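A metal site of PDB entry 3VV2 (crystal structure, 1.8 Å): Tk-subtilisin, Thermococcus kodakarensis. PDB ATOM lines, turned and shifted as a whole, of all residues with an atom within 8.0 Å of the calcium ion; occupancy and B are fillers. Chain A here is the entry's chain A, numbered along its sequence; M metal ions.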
ATOM      1  N   VAL A  49      -9.758 -23.562 -16.755  1.00  0.00           N
ATOM      2  CA  VAL A  49     -10.213 -23.503 -18.133  1.00  0.00           C
ATOM      3  C   VAL A  49      -9.864 -24.687 -19.034  1.00  0.00           C
ATOM      4  O   VAL A  49      -8.862 -25.325 -18.895  1.00  0.00           O
ATOM      5  CB  VAL A  49      -9.728 -22.209 -18.826  1.00  0.00           C
ATOM      6  CG1 VAL A  49      -8.236 -22.268 -19.084  1.00  0.00           C
ATOM      7  CG2 VAL A  49     -10.529 -21.940 -20.077  1.00  0.00           C
ATOM      8  N   ASP A  50     -10.785 -24.920 -19.945  1.00  0.00           N
ATOM      9  CA  ASP A  50     -10.567 -25.982 -20.906  1.00  0.00           C
ATOM     10  C   ASP A  50      -9.638 -25.327 -21.913  1.00  0.00           C
ATOM     11  O   ASP A  50     -10.046 -24.711 -22.864  1.00  0.00           O
ATOM     12  CB  ASP A  50     -11.935 -26.437 -21.423  1.00  0.00           C
ATOM     13  CG  ASP A  50     -11.812 -27.471 -22.565  1.00  0.00           C
ATOM     14  OD1 ASP A  50     -12.799 -27.859 -23.171  1.00  0.00           O
ATOM     15  OD2 ASP A  50     -10.685 -27.810 -22.828  1.00  0.00           O
ATOM     16  N   TYR A  51      -8.325 -25.374 -21.647  1.00  0.00           N
ATOM     17  CA  TYR A  51      -7.453 -24.408 -22.321  1.00  0.00           C
ATOM     18  C   TYR A  51      -7.339 -24.685 -23.779  1.00  0.00           C
ATOM     19  O   TYR A  51      -6.872 -23.802 -24.523  1.00  0.00           O
ATOM     20  CB  TYR A  51      -6.035 -24.316 -21.702  1.00  0.00           C
ATOM     21  CG  TYR A  51      -5.371 -25.656 -21.606  1.00  0.00           C
ATOM     22  CD1 TYR A  51      -5.323 -26.368 -20.404  1.00  0.00           C
ATOM     23  CD2 TYR A  51      -4.719 -26.202 -22.732  1.00  0.00           C
ATOM     24  CE1 TYR A  51      -4.690 -27.606 -20.318  1.00  0.00           C
ATOM     25  CE2 TYR A  51      -4.074 -27.438 -22.657  1.00  0.00           C
ATOM     26  CZ  TYR A  51      -4.059 -28.125 -21.459  1.00  0.00           C
ATOM     27  OH  TYR A  51      -3.425 -29.329 -21.397  1.00  0.00           O
ATOM     28  N   ASP A  52      -7.721 -25.842 -24.214  1.00  0.00           N
ATOM     29  CA  ASP A  52      -7.616 -26.227 -25.613  1.00  0.00           C
ATOM     30  C   ASP A  52      -8.926 -26.058 -26.388  1.00  0.00           C
ATOM     31  O   ASP A  52      -8.986 -26.406 -27.570  1.00  0.00           O
ATOM     32  CB  ASP A  52      -7.124 -27.676 -25.729  1.00  0.00           C
ATOM     33  CG  ASP A  52      -8.146 -28.685 -25.244  1.00  0.00           C
ATOM     34  OD1 ASP A  52      -9.031 -29.060 -26.038  1.00  0.00           O
ATOM     35  OD2 ASP A  52      -8.059 -29.094 -24.073  1.00  0.00           O
ATOM     36  N   HIS A  53     -10.009 -25.558 -25.738  1.00  0.00           N
ATOM     37  CA  HIS A  53     -11.254 -25.377 -26.423  1.00  0.00           C
ATOM     38  C   HIS A  53     -11.080 -24.584 -27.676  1.00  0.00           C
ATOM     39  O   HIS A  53     -10.406 -23.557 -27.689  1.00  0.00           O
ATOM     40  CB  HIS A  53     -12.262 -24.645 -25.524  1.00  0.00           C
ATOM     41  CG  HIS A  53     -13.672 -24.712 -26.026  1.00  0.00           C
ATOM     42  ND1 HIS A  53     -14.682 -25.315 -25.308  1.00  0.00           N
ATOM     43  CD2 HIS A  53     -14.257 -24.179 -27.118  1.00  0.00           C
ATOM     44  CE1 HIS A  53     -15.828 -25.196 -25.962  1.00  0.00           C
ATOM     45  NE2 HIS A  53     -15.591 -24.497 -27.066  1.00  0.00           N
ATOM     46  N   PRO A  54     -11.722 -25.051 -28.773  1.00  0.00           N
ATOM     47  CA  PRO A  54     -11.510 -24.320 -30.025  1.00  0.00           C
ATOM     48  C   PRO A  54     -12.060 -22.861 -30.021  1.00  0.00           C
ATOM     49  O   PRO A  54     -11.588 -22.051 -30.794  1.00  0.00           O
ATOM     50  CB  PRO A  54     -12.288 -25.150 -31.039  1.00  0.00           C
ATOM     51  CG  PRO A  54     -12.145 -26.547 -30.546  1.00  0.00           C
ATOM     52  CD  PRO A  54     -12.326 -26.360 -29.011  1.00  0.00           C
ATOM     53  N   THR A  86     -14.724 -22.562 -17.470  1.00  0.00           N
ATOM     54  CA  THR A  86     -14.757 -22.492 -18.907  1.00  0.00           C
ATOM     55  C   THR A  86     -16.018 -21.723 -19.396  1.00  0.00           C
ATOM     56  O   THR A  86     -15.974 -20.965 -20.351  1.00  0.00           O
ATOM     57  CB  THR A  86     -14.775 -23.958 -19.455  1.00  0.00           C
ATOM     58  OG1 THR A  86     -13.581 -24.625 -19.021  1.00  0.00           O
ATOM     59  CG2 THR A  86     -14.827 -23.986 -20.963  1.00  0.00           C
ATOM     60  N   TYR A 243     -17.986 -25.074 -22.606  1.00  0.00           N
ATOM     61  CA  TYR A 243     -18.061 -26.052 -21.524  1.00  0.00           C
ATOM     62  C   TYR A 243     -17.177 -27.222 -21.898  1.00  0.00           C
ATOM     63  O   TYR A 243     -17.028 -27.476 -23.107  1.00  0.00           O
ATOM     64  CB  TYR A 243     -19.483 -26.531 -21.357  1.00  0.00           C
ATOM     65  CG  TYR A 243     -19.770 -26.963 -19.965  1.00  0.00           C
ATOM     66  CD1 TYR A 243     -19.851 -26.030 -18.914  1.00  0.00           C
ATOM     67  CD2 TYR A 243     -19.981 -28.311 -19.687  1.00  0.00           C
ATOM     68  CE1 TYR A 243     -20.144 -26.476 -17.618  1.00  0.00           C
ATOM     69  CE2 TYR A 243     -20.273 -28.734 -18.437  1.00  0.00           C
ATOM     70  CZ  TYR A 243     -20.360 -27.824 -17.414  1.00  0.00           C
ATOM     71  OH  TYR A 243     -20.590 -28.356 -16.176  1.00  0.00           O
ATOM     72  N   PRO A 244     -16.514 -27.881 -20.907  1.00  0.00           N
ATOM     73  CA  PRO A 244     -15.643 -29.048 -21.278  1.00  0.00           C
ATOM     74  C   PRO A 244     -16.441 -30.235 -21.841  1.00  0.00           C
ATOM     75  O   PRO A 244     -17.605 -30.423 -21.462  1.00  0.00           O
ATOM     76  CB  PRO A 244     -15.046 -29.495 -19.962  1.00  0.00           C
ATOM     77  CG  PRO A 244     -15.169 -28.224 -18.994  1.00  0.00           C
ATOM     78  CD  PRO A 244     -16.393 -27.486 -19.486  1.00  0.00           C
ATOM     79  N   ASP A 245     -15.834 -31.026 -22.730  1.00  0.00           N
ATOM     80  CA  ASP A 245     -14.501 -30.750 -23.248  1.00  0.00           C
ATOM     81  C   ASP A 245     -14.599 -30.364 -24.722  1.00  0.00           C
ATOM     82  O   ASP A 245     -14.858 -31.211 -25.576  1.00  0.00           O
ATOM     83  CB  ASP A 245     -13.603 -31.974 -23.079  1.00  0.00           C
ATOM     84  CG  ASP A 245     -12.139 -31.654 -23.317  1.00  0.00           C
ATOM     85  OD1 ASP A 245     -11.796 -31.250 -24.450  1.00  0.00           O
ATOM     86  OD2 ASP A 245     -11.334 -31.801 -22.376  1.00  0.00           O
ATOM     87  N   ASP A 246     -14.390 -29.087 -25.002  1.00  0.00           N
ATOM     88  CA  ASP A 246     -14.538 -28.544 -26.318  1.00  0.00           C
ATOM     89  C   ASP A 246     -16.010 -28.531 -26.755  1.00  0.00           C
ATOM     90  O   ASP A 246     -16.313 -28.684 -27.943  1.00  0.00           O
ATOM     91  CB  ASP A 246     -13.615 -29.319 -27.302  1.00  0.00           C
ATOM     92  CG  ASP A 246     -12.233 -29.604 -26.719  1.00  0.00           C
ATOM     93  OD1 ASP A 246     -11.877 -29.051 -25.617  1.00  0.00           O
ATOM     94  OD2 ASP A 246     -11.493 -30.429 -27.336  1.00  0.00           O
ATOM     95  N   SER A 247     -16.908 -28.360 -25.780  1.00  0.00           N
ATOM     96  CA  SER A 247     -18.369 -28.331 -25.996  1.00  0.00           C
ATOM     97  C   SER A 247     -19.063 -27.191 -25.165  1.00  0.00           C
ATOM     98  O   SER A 247     -18.385 -26.361 -24.552  1.00  0.00           O
ATOM     99  CB  SER A 247     -19.005 -29.630 -25.414  1.00  0.00           C
ATOM    100  OG  SER A 247     -20.433 -29.659 -25.514  1.00  0.00           O
HETATM  101 CA    CA M   1     -10.585 -29.246 -24.412  1.00  0.00          CA
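The backbone NH (N) of Asp 50 is in hydrogen-bond range of the side-chain hydroxyl (OG1) of Thr 86 (3.0 Å).
His 53 touches the calcium ion (N to CA, 3.96 Å). Within 4 Å of the calcium ion: Asp 50, Asp 52, His 53, Asp 245 and Asp 246. The nearest printed residue that does not touch the calcium ion is Tyr 51 (5.3 Å).
The calcium ion is bound by OD1 of Asp 246, at 1.8 Å. OD2 of Asp 50 is bound to the calcium ion. OD1 of Asp 52 binds the calcium ion, 2.3 Å away. The side-chain carboxylate (OD1) of Asp 245 is bound to the calcium ion, 2.3 Å away. The calcium ion is bound by OD2 of Asp 52, at 2.6 Å. The side-chain carboxylate (OD1) of Asp 50 is bound to the calcium ion, 2.9 Å away. The calcium ion has six donor atoms within binding distance.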
